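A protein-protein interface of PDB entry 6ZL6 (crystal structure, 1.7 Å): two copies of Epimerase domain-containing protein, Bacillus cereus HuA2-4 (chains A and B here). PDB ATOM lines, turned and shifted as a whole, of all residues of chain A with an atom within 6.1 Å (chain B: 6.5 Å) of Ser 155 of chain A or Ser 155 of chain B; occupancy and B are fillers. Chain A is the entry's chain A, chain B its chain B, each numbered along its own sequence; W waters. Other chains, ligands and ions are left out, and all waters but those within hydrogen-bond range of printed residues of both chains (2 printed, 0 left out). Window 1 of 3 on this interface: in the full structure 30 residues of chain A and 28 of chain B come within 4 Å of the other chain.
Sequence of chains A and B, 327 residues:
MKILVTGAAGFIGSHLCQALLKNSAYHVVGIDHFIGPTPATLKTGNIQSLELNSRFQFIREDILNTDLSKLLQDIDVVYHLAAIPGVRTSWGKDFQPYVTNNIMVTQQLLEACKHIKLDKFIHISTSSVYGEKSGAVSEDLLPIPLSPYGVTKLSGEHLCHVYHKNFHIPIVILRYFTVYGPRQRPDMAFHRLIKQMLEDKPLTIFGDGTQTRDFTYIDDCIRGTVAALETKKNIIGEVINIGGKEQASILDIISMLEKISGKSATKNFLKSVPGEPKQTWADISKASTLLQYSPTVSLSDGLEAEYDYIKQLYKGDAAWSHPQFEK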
ATOM      1  N   PHE A  95      10.306  11.612 -24.627  1.00  0.00           N
ATOM      2  CA  PHE A  95       8.940  11.627 -24.042  1.00  0.00           C
ATOM      3  C   PHE A  95       8.796  12.630 -22.895  1.00  0.00           C
ATOM      4  O   PHE A  95       7.693  13.274 -22.791  1.00  0.00           O
ATOM      5  CB  PHE A  95       8.589  10.243 -23.476  1.00  0.00           C
ATOM      6  CG  PHE A  95       7.202  10.074 -22.895  1.00  0.00           C
ATOM      7  CD1 PHE A  95       6.060  10.311 -23.652  1.00  0.00           C
ATOM      8  CD2 PHE A  95       7.043   9.577 -21.614  1.00  0.00           C
ATOM      9  CE1 PHE A  95       4.783  10.099 -23.117  1.00  0.00           C
ATOM     10  CE2 PHE A  95       5.776   9.365 -21.076  1.00  0.00           C
ATOM     11  CZ  PHE A  95       4.651   9.590 -21.834  1.00  0.00           C
ATOM     12  N   ASN A 102       2.621  18.928 -21.714  1.00  0.00           N
ATOM     13  CA  ASN A 102       1.234  18.569 -22.078  1.00  0.00           C
ATOM     14  C   ASN A 102       0.462  18.197 -20.808  1.00  0.00           C
ATOM     15  O   ASN A 102      -0.713  18.460 -20.810  1.00  0.00           O
ATOM     16  CB  ASN A 102       1.168  17.496 -23.169  1.00  0.00           C
ATOM     17  CG  ASN A 102       1.880  17.903 -24.445  1.00  0.00           C
ATOM     18  OD1 ASN A 102       2.281  19.055 -24.614  1.00  0.00           O
ATOM     19  ND2 ASN A 102       2.053  16.963 -25.361  1.00  0.00           N
ATOM     20  N   ILE A 103       1.094  17.618 -19.785  1.00  0.00           N
ATOM     21  CA  ILE A 103       0.329  17.170 -18.592  1.00  0.00           C
ATOM     22  C   ILE A 103       0.571  18.160 -17.459  1.00  0.00           C
ATOM     23  O   ILE A 103      -0.396  18.693 -16.938  1.00  0.00           O
ATOM     24  CB  ILE A 103       0.671  15.721 -18.202  1.00  0.00           C
ATOM     25  CG1 ILE A 103       0.416  14.764 -19.367  1.00  0.00           C
ATOM     26  CG2 ILE A 103      -0.107  15.283 -16.982  1.00  0.00           C
ATOM     27  CD1 ILE A 103       0.879  13.343 -19.109  1.00  0.00           C
ATOM     28  N   THR A 106      -0.845  21.683 -18.041  1.00  0.00           N
ATOM     29  CA  THR A 106      -2.328  21.735 -18.010  1.00  0.00           C
ATOM     30  C   THR A 106      -2.784  21.701 -16.533  1.00  0.00           C
ATOM     31  O   THR A 106      -3.642  22.502 -16.155  1.00  0.00           O
ATOM     32  CB  THR A 106      -2.906  20.629 -18.882  1.00  0.00           C
ATOM     33  OG1 THR A 106      -2.444  20.843 -20.216  1.00  0.00           O
ATOM     34  CG2 THR A 106      -4.416  20.579 -18.853  1.00  0.00           C
ATOM     35  N   GLY A 150      -0.173  11.430 -28.369  1.00  0.00           N
ATOM     36  CA  GLY A 150      -1.637  11.295 -28.203  1.00  0.00           C
ATOM     37  C   GLY A 150      -2.037  10.959 -26.760  1.00  0.00           C
ATOM     38  O   GLY A 150      -3.010  11.540 -26.258  1.00  0.00           O
ATOM     39  N   VAL A 151      -1.313  10.051 -26.109  1.00  0.00           N
ATOM     40  CA  VAL A 151      -1.555   9.743 -24.670  1.00  0.00           C
ATOM     41  C   VAL A 151      -1.467  11.045 -23.837  1.00  0.00           C
ATOM     42  O   VAL A 151      -2.336  11.224 -22.973  1.00  0.00           O
ATOM     43  CB  VAL A 151      -0.565   8.710 -24.143  1.00  0.00           C
ATOM     44  CG1 VAL A 151      -0.680   8.606 -22.630  1.00  0.00           C
ATOM     45  CG2 VAL A 151      -0.728   7.378 -24.863  1.00  0.00           C
ATOM     46  N   THR A 152      -0.408  11.849 -23.988  1.00  0.00           N
ATOM     47  CA  THR A 152      -0.201  13.057 -23.129  1.00  0.00           C
ATOM     48  C   THR A 152      -1.327  14.079 -23.401  1.00  0.00           C
ATOM     49  O   THR A 152      -1.780  14.673 -22.479  1.00  0.00           O
ATOM     50  CB  THR A 152       1.211  13.674 -23.227  1.00  0.00           C
ATOM     51  OG1 THR A 152       1.433  14.150 -24.559  1.00  0.00           O
ATOM     52  CG2 THR A 152       2.291  12.695 -22.796  1.00  0.00           C
ATOM     53  N   LYS A 153      -1.766  14.231 -24.646  1.00  0.00           N
ATOM     54  CA  LYS A 153      -2.863  15.159 -24.998  1.00  0.00           C
ATOM     55  C   LYS A 153      -4.153  14.654 -24.353  1.00  0.00           C
ATOM     56  O   LYS A 153      -4.900  15.459 -23.826  1.00  0.00           O
ATOM     57  CB  LYS A 153      -2.913  15.330 -26.509  1.00  0.00           C
ATOM     58  CG  LYS A 153      -1.738  16.157 -27.030  1.00  0.00           C
ATOM     59  CD  LYS A 153      -1.743  17.632 -26.586  1.00  0.00           C
ATOM     60  CE  LYS A 153      -2.927  18.402 -27.162  1.00  0.00           C
ATOM     61  NZ  LYS A 153      -2.882  19.846 -26.845  1.00  0.00           N
ATOM     62  N   LEU A 154      -4.387  13.339 -24.378  1.00  0.00           N
ATOM     63  CA  LEU A 154      -5.616  12.794 -23.783  1.00  0.00           C
ATOM     64  C   LEU A 154      -5.550  13.000 -22.274  1.00  0.00           C
ATOM     65  O   LEU A 154      -6.592  13.417 -21.702  1.00  0.00           O
ATOM     66  CB  LEU A 154      -5.780  11.324 -24.165  1.00  0.00           C
ATOM     67  CG  LEU A 154      -7.085  10.675 -23.736  1.00  0.00           C
ATOM     68  CD1 LEU A 154      -8.295  11.502 -24.194  1.00  0.00           C
ATOM     69  CD2 LEU A 154      -7.123   9.238 -24.243  1.00  0.00           C
ATOM     70  N   SER A 155      -4.367  12.880 -21.647  1.00  0.00           N
ATOM     71  CA  SER A 155      -4.258  13.114 -20.178  1.00  0.00           C
ATOM     72  C   SER A 155      -4.636  14.568 -19.866  1.00  0.00           C
ATOM     73  O   SER A 155      -5.267  14.815 -18.827  1.00  0.00           O
ATOM     74  CB  SER A 155      -2.906  12.723 -19.618  1.00  0.00           C
ATOM     75  OG  SER A 155      -2.708  11.339 -19.864  1.00  0.00           O
ATOM     76  N   GLY A 156      -4.262  15.501 -20.739  1.00  0.00           N
ATOM     77  CA  GLY A 156      -4.660  16.923 -20.635  1.00  0.00           C
ATOM     78  C   GLY A 156      -6.171  17.101 -20.599  1.00  0.00           C
ATOM     79  O   GLY A 156      -6.692  17.858 -19.718  1.00  0.00           O
ATOM     80  N   GLU A 157      -6.866  16.467 -21.526  1.00  0.00           N
ATOM     81  CA  GLU A 157      -8.338  16.523 -21.622  1.00  0.00           C
ATOM     82  C   GLU A 157      -8.907  16.001 -20.305  1.00  0.00           C
ATOM     83  O   GLU A 157      -9.835  16.595 -19.796  1.00  0.00           O
ATOM     84  CB  GLU A 157      -8.892  15.646 -22.730  1.00  0.00           C
ATOM     85  CG  GLU A 157      -8.535  16.117 -24.128  1.00  0.00           C
ATOM     86  CD  GLU A 157      -9.365  15.406 -25.186  1.00  0.00           C
ATOM     87  OE1 GLU A 157     -10.372  14.727 -24.808  1.00  0.00           O
ATOM     88  OE2 GLU A 157      -9.001  15.513 -26.358  1.00  0.00           O
ATOM     89  N   HIS A 158      -8.366  14.887 -19.818  1.00  0.00           N
ATOM     90  CA  HIS A 158      -8.874  14.211 -18.594  1.00  0.00           C
ATOM     91  C   HIS A 158      -8.678  15.137 -17.402  1.00  0.00           C
ATOM     92  O   HIS A 158      -9.646  15.240 -16.579  1.00  0.00           O
ATOM     93  CB  HIS A 158      -8.234  12.837 -18.410  1.00  0.00           C
ATOM     94  CG  HIS A 158      -8.688  11.803 -19.382  1.00  0.00           C
ATOM     95  ND1 HIS A 158      -7.888  10.728 -19.694  1.00  0.00           N
ATOM     96  CD2 HIS A 158      -9.798  11.688 -20.138  1.00  0.00           C
ATOM     97  CE1 HIS A 158      -8.539   9.948 -20.547  1.00  0.00           C
ATOM     98  NE2 HIS A 158      -9.688  10.525 -20.845  1.00  0.00           N
ATOM     99  N   LEU A 159      -7.552  15.855 -17.317  1.00  0.00           N
ATOM    100  CA  LEU A 159      -7.364  16.838 -16.225  1.00  0.00           C
ATOM    101  C   LEU A 159      -8.467  17.900 -16.354  1.00  0.00           C
ATOM    102  O   LEU A 159      -9.003  18.284 -15.313  1.00  0.00           O
ATOM    103  CB  LEU A 159      -5.984  17.474 -16.280  1.00  0.00           C
ATOM    104  CG  LEU A 159      -4.835  16.586 -15.825  1.00  0.00           C
ATOM    105  CD1 LEU A 159      -3.515  17.149 -16.279  1.00  0.00           C
ATOM    106  CD2 LEU A 159      -4.833  16.385 -14.322  1.00  0.00           C
ATOM    107  N   CYS A 160      -8.798  18.346 -17.568  1.00  0.00           N
ATOM    108  CA  CYS A 160      -9.877  19.367 -17.768  1.00  0.00           C
ATOM    109  C   CYS A 160     -11.198  18.871 -17.150  1.00  0.00           C
ATOM    110  O   CYS A 160     -11.814  19.618 -16.344  1.00  0.00           O
ATOM    111  CB  CYS A 160     -10.069  19.698 -19.236  1.00  0.00           C
ATOM    112  SG  CYS A 160      -8.769  20.762 -19.883  1.00  0.00           S
ATOM    113  N   ASN B 102       3.795   7.163 -12.021  1.00  0.00           N
ATOM    114  CA  ASN B 102       2.667   6.429 -12.626  1.00  0.00           C
ATOM    115  C   ASN B 102       2.805   6.516 -14.144  1.00  0.00           C
ATOM    116  O   ASN B 102       2.398   5.545 -14.836  1.00  0.00           O
ATOM    117  CB  ASN B 102       1.281   6.877 -12.164  1.00  0.00           C
ATOM    118  CG  ASN B 102       1.081   6.744 -10.669  1.00  0.00           C
ATOM    119  OD1 ASN B 102       1.886   6.103  -9.998  1.00  0.00           O
ATOM    120  ND2 ASN B 102      -0.014   7.268 -10.144  1.00  0.00           N
ATOM    121  N   ILE B 103       3.322   7.634 -14.660  1.00  0.00           N
ATOM    122  CA  ILE B 103       3.466   7.797 -16.118  1.00  0.00           C
ATOM    123  C   ILE B 103       4.915   7.513 -16.509  1.00  0.00           C
ATOM    124  O   ILE B 103       5.105   6.672 -17.365  1.00  0.00           O
ATOM    125  CB  ILE B 103       2.967   9.176 -16.585  1.00  0.00           C
ATOM    126  CG1 ILE B 103       1.535   9.413 -16.083  1.00  0.00           C
ATOM    127  CG2 ILE B 103       3.076   9.246 -18.099  1.00  0.00           C
ATOM    128  CD1 ILE B 103       0.874  10.651 -16.596  1.00  0.00           C
ATOM    129  N   THR B 106       6.105   3.897 -15.942  1.00  0.00           N
ATOM    130  CA  THR B 106       5.488   2.965 -16.911  1.00  0.00           C
ATOM    131  C   THR B 106       6.166   3.110 -18.283  1.00  0.00           C
ATOM    132  O   THR B 106       6.542   2.090 -18.891  1.00  0.00           O
ATOM    133  CB  THR B 106       3.973   3.169 -16.944  1.00  0.00           C
ATOM    134  OG1 THR B 106       3.459   2.939 -15.634  1.00  0.00           O
ATOM    135  CG2 THR B 106       3.284   2.249 -17.912  1.00  0.00           C
ATOM    136  N   VAL B 129      -9.948   4.792 -12.920  1.00  0.00           N
ATOM    137  CA  VAL B 129      -9.970   5.317 -14.314  1.00  0.00           C
ATOM    138  C   VAL B 129     -11.423   5.596 -14.757  1.00  0.00           C
ATOM    139  O   VAL B 129     -11.608   6.406 -15.639  1.00  0.00           O
ATOM    140  CB  VAL B 129      -9.228   4.398 -15.291  1.00  0.00           C
ATOM    141  CG1 VAL B 129      -7.790   4.130 -14.825  1.00  0.00           C
ATOM    142  CG2 VAL B 129      -9.993   3.123 -15.532  1.00  0.00           C
ATOM    143  N   GLY B 150      -6.436   9.092 -10.838  1.00  0.00           N
ATOM    144  CA  GLY B 150      -7.114   8.349 -11.910  1.00  0.00           C
ATOM    145  C   GLY B 150      -6.599   8.732 -13.285  1.00  0.00           C
ATOM    146  O   GLY B 150      -6.456   7.860 -14.138  1.00  0.00           O
ATOM    147  N   VAL B 151      -6.355  10.014 -13.543  1.00  0.00           N
ATOM    148  CA  VAL B 151      -5.822  10.467 -14.871  1.00  0.00           C
ATOM    149  C   VAL B 151      -4.463   9.774 -15.100  1.00  0.00           C
ATOM    150  O   VAL B 151      -4.223   9.259 -16.201  1.00  0.00           O
ATOM    151  CB  VAL B 151      -5.657  11.988 -14.890  1.00  0.00           C
ATOM    152  CG1 VAL B 151      -4.920  12.464 -16.129  1.00  0.00           C
ATOM    153  CG2 VAL B 151      -7.010  12.675 -14.746  1.00  0.00           C
ATOM    154  N   THR B 152      -3.588   9.782 -14.095  1.00  0.00           N
ATOM    155  CA  THR B 152      -2.202   9.251 -14.253  1.00  0.00           C
ATOM    156  C   THR B 152      -2.255   7.743 -14.504  1.00  0.00           C
ATOM    157  O   THR B 152      -1.449   7.253 -15.294  1.00  0.00           O
ATOM    158  CB  THR B 152      -1.250   9.638 -13.115  1.00  0.00           C
ATOM    159  OG1 THR B 152      -1.658   9.015 -11.898  1.00  0.00           O
ATOM    160  CG2 THR B 152      -1.124  11.142 -12.982  1.00  0.00           C
ATOM    161  N   LYS B 153      -3.155   7.020 -13.842  1.00  0.00           N
ATOM    162  CA  LYS B 153      -3.227   5.555 -14.018  1.00  0.00           C
ATOM    163  C   LYS B 153      -3.793   5.267 -15.415  1.00  0.00           C
ATOM    164  O   LYS B 153      -3.335   4.330 -16.091  1.00  0.00           O
ATOM    165  CB  LYS B 153      -4.043   4.964 -12.862  1.00  0.00           C
ATOM    166  CG  LYS B 153      -3.342   5.001 -11.512  1.00  0.00           C
ATOM    167  CD  LYS B 153      -2.158   4.068 -11.342  1.00  0.00           C
ATOM    168  CE  LYS B 153      -2.508   2.585 -11.436  1.00  0.00           C
ATOM    169  NZ  LYS B 153      -1.333   1.755 -11.110  1.00  0.00           N
ATOM    170  N   LEU B 154      -4.763   6.050 -15.862  1.00  0.00           N
ATOM    171  CA  LEU B 154      -5.335   5.800 -17.199  1.00  0.00           C
ATOM    172  C   LEU B 154      -4.247   6.123 -18.240  1.00  0.00           C
ATOM    173  O   LEU B 154      -4.149   5.433 -19.216  1.00  0.00           O
ATOM    174  CB  LEU B 154      -6.623   6.612 -17.381  1.00  0.00           C
ATOM    175  CG  LEU B 154      -7.326   6.401 -18.714  1.00  0.00           C
ATOM    176  CD1 LEU B 154      -7.630   4.927 -18.953  1.00  0.00           C
ATOM    177  CD2 LEU B 154      -8.584   7.270 -18.789  1.00  0.00           C
ATOM    178  N   SER B 155      -3.398   7.113 -18.002  1.00  0.00           N
ATOM    179  CA  SER B 155      -2.298   7.426 -18.956  1.00  0.00           C
ATOM    180  C   SER B 155      -1.355   6.201 -19.054  1.00  0.00           C
ATOM    181  O   SER B 155      -0.897   5.876 -20.163  1.00  0.00           O
ATOM    182  CB  SER B 155      -1.626   8.681 -18.496  1.00  0.00           C
ATOM    183  OG  SER B 155      -0.709   9.187 -19.436  1.00  0.00           O
ATOM    184  N   GLY B 156      -1.050   5.557 -17.929  1.00  0.00           N
ATOM    185  CA  GLY B 156      -0.246   4.316 -17.931  1.00  0.00           C
ATOM    186  C   GLY B 156      -0.882   3.222 -18.768  1.00  0.00           C
ATOM    187  O   GLY B 156      -0.157   2.562 -19.546  1.00  0.00           O
ATOM    188  N   GLU B 157      -2.182   2.999 -18.617  1.00  0.00           N
ATOM    189  CA  GLU B 157      -2.904   2.028 -19.466  1.00  0.00           C
ATOM    190  C   GLU B 157      -2.677   2.383 -20.930  1.00  0.00           C
ATOM    191  O   GLU B 157      -2.308   1.520 -21.732  1.00  0.00           O
ATOM    192  CB  GLU B 157      -4.410   2.024 -19.239  1.00  0.00           C
ATOM    193  CG  GLU B 157      -4.837   1.538 -17.876  1.00  0.00           C
ATOM    194  CD  GLU B 157      -6.319   1.176 -17.757  1.00  0.00           C
ATOM    195  OE1 GLU B 157      -6.938   0.983 -18.822  1.00  0.00           O
ATOM    196  OE2 GLU B 157      -6.843   1.035 -16.589  1.00  0.00           O
ATOM    197  N   HIS B 158      -2.893   3.645 -21.277  1.00  0.00           N
ATOM    198  CA  HIS B 158      -2.752   4.074 -22.683  1.00  0.00           C
ATOM    199  C   HIS B 158      -1.337   3.868 -23.203  1.00  0.00           C
ATOM    200  O   HIS B 158      -1.202   3.442 -24.375  1.00  0.00           O
ATOM    201  CB  HIS B 158      -3.180   5.521 -22.816  1.00  0.00           C
ATOM    202  CG  HIS B 158      -4.639   5.687 -22.688  1.00  0.00           C
ATOM    203  ND1 HIS B 158      -5.197   6.881 -22.238  1.00  0.00           N
ATOM    204  CD2 HIS B 158      -5.663   4.837 -22.863  1.00  0.00           C
ATOM    205  CE1 HIS B 158      -6.511   6.737 -22.206  1.00  0.00           C
ATOM    206  NE2 HIS B 158      -6.820   5.531 -22.587  1.00  0.00           N
ATOM    207  N   LEU B 159      -0.319   4.123 -22.385  1.00  0.00           N
ATOM    208  CA  LEU B 159       1.074   3.778 -22.756  1.00  0.00           C
ATOM    209  C   LEU B 159       1.198   2.278 -23.022  1.00  0.00           C
ATOM    210  O   LEU B 159       1.811   1.902 -24.041  1.00  0.00           O
ATOM    211  CB  LEU B 159       2.040   4.219 -21.678  1.00  0.00           C
ATOM    212  CG  LEU B 159       2.277   5.726 -21.600  1.00  0.00           C
ATOM    213  CD1 LEU B 159       2.948   6.088 -20.299  1.00  0.00           C
ATOM    214  CD2 LEU B 159       3.064   6.199 -22.812  1.00  0.00           C
ATOM    215  N   CYS B 160       0.580   1.421 -22.217  1.00  0.00           N
ATOM    216  CA  CYS B 160       0.603  -0.045 -22.510  1.00  0.00           C
ATOM    217  C   CYS B 160       0.059  -0.313 -23.927  1.00  0.00           C
ATOM    218  O   CYS B 160       0.683  -1.103 -24.656  1.00  0.00           O
ATOM    219  CB  CYS B 160      -0.145  -0.862 -21.464  1.00  0.00           C
ATOM    220  SG  CYS B 160       0.709  -0.891 -19.861  1.00  0.00           S
HETATM  221  O   HOH W   1      -5.223   9.894 -18.890  1.00  0.00           O
HETATM  222  O   HOH W   2      -3.971   9.424 -21.379  1.00  0.00           O
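Among the printed residues, merely in contact across the chains: Phe 95 of chain A with Leu 159 of chain B (3.9 Å), Ile 103 of chain A with Ile 103 of chain B (3.7 Å), Val 151 of chain A with Ser 155 of chain B (3.2 Å), Val 151 of chain A with His 158 of chain B (3.7 Å), Leu 154 of chain A with His 158 of chain B (3.3 Å), Ser 155 of chain A with Val 151 of chain B (3.6 Å), His 158 of chain A with Val 151 of chain B (3.9 Å) and His 158 of chain A with Leu 154 of chain B (3.2 Å).
Val 151 of chain A touches Ser 155 of chain B, and with the chains exchanged Ser 155 of chain A touches Val 151 of chain B.
Val 151 of chain A touches His 158 of chain B, and with the chains exchanged His 158 of chain A touches Val 151 of chain B.
Leu 154 of chain A touches His 158 of chain B, and with the chains exchanged His 158 of chain A touches Leu 154 of chain B.
Ser 155 of chain A touches its own counterpart, Ser 155 of chain B.
14 positions are printed for both chains.
Of the 9 pairs that touch across the chains among the printed residues, 8 have their exchanged pair printed and touching as well.
O of Val 151 of chain A lies within hydrogen-bond range of OG of Ser 155 of chain A (3.1 Å).
Hydrophobic or aromatic side chains of chain A within 4 Å of the printed part of chain B: Phe 95, Ile 103, Val 151, Leu 154 and His 158.
Along chain A the printed residues that touch a printed residue of chain B span positions 95 to 158.
Of the 15 printed residues of chain B, 6 touch a printed residue of chain A.
Among the printed residues, 9 pairs touch across the chains.
Among the printed residues, no Asp or Glu carboxylate lies within 4 Å of a Lys or Arg side-chain nitrogen of the other chain.
Of chain B, only Val 151 and Ser 155 come within 4 Å of Ser 155 of chain A.
Ser 155 of chain B touches just these residues of chain A: Val 151 and Ser 155.
Of the printed residues of chain A, Leu 159 of chain B touches Phe 95 (3.9 Å).
Of the printed residues of chain A, Leu 154 of chain B touches His 158 (3.2 Å).
Printed residues of chain B within 4 Å of Ile 103 of chain A: Ile 103.
The nearest residue of chain B that does not touch Ser 155 of chain A is Ile 103 of chain B (4.9 Å).
The side-chain hydroxyl (OG) of Ser 155 of chain A lies within hydrogen-bond range of the side-chain hydroxyl (OG) of Ser 155 of chain B (3.0 Å).
Water W2 lies within hydrogen-bond range of the side-chain hydroxyl of Ser 155 of chain A (2.7 Å), the backbone carbonyl oxygen of Val 151 of chain A (2.9 Å) and a ring nitrogen (ND1) of His 158 of chain B (3.0 Å).
Water W1 lies within hydrogen-bond range of a ring nitrogen (ND1) of His 158 of chain A, the backbone carbonyl oxygen of Val 151 of chain B, the side-chain hydroxyl of Ser 155 of chain A and the backbone NH of Ser 155 of chain B.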
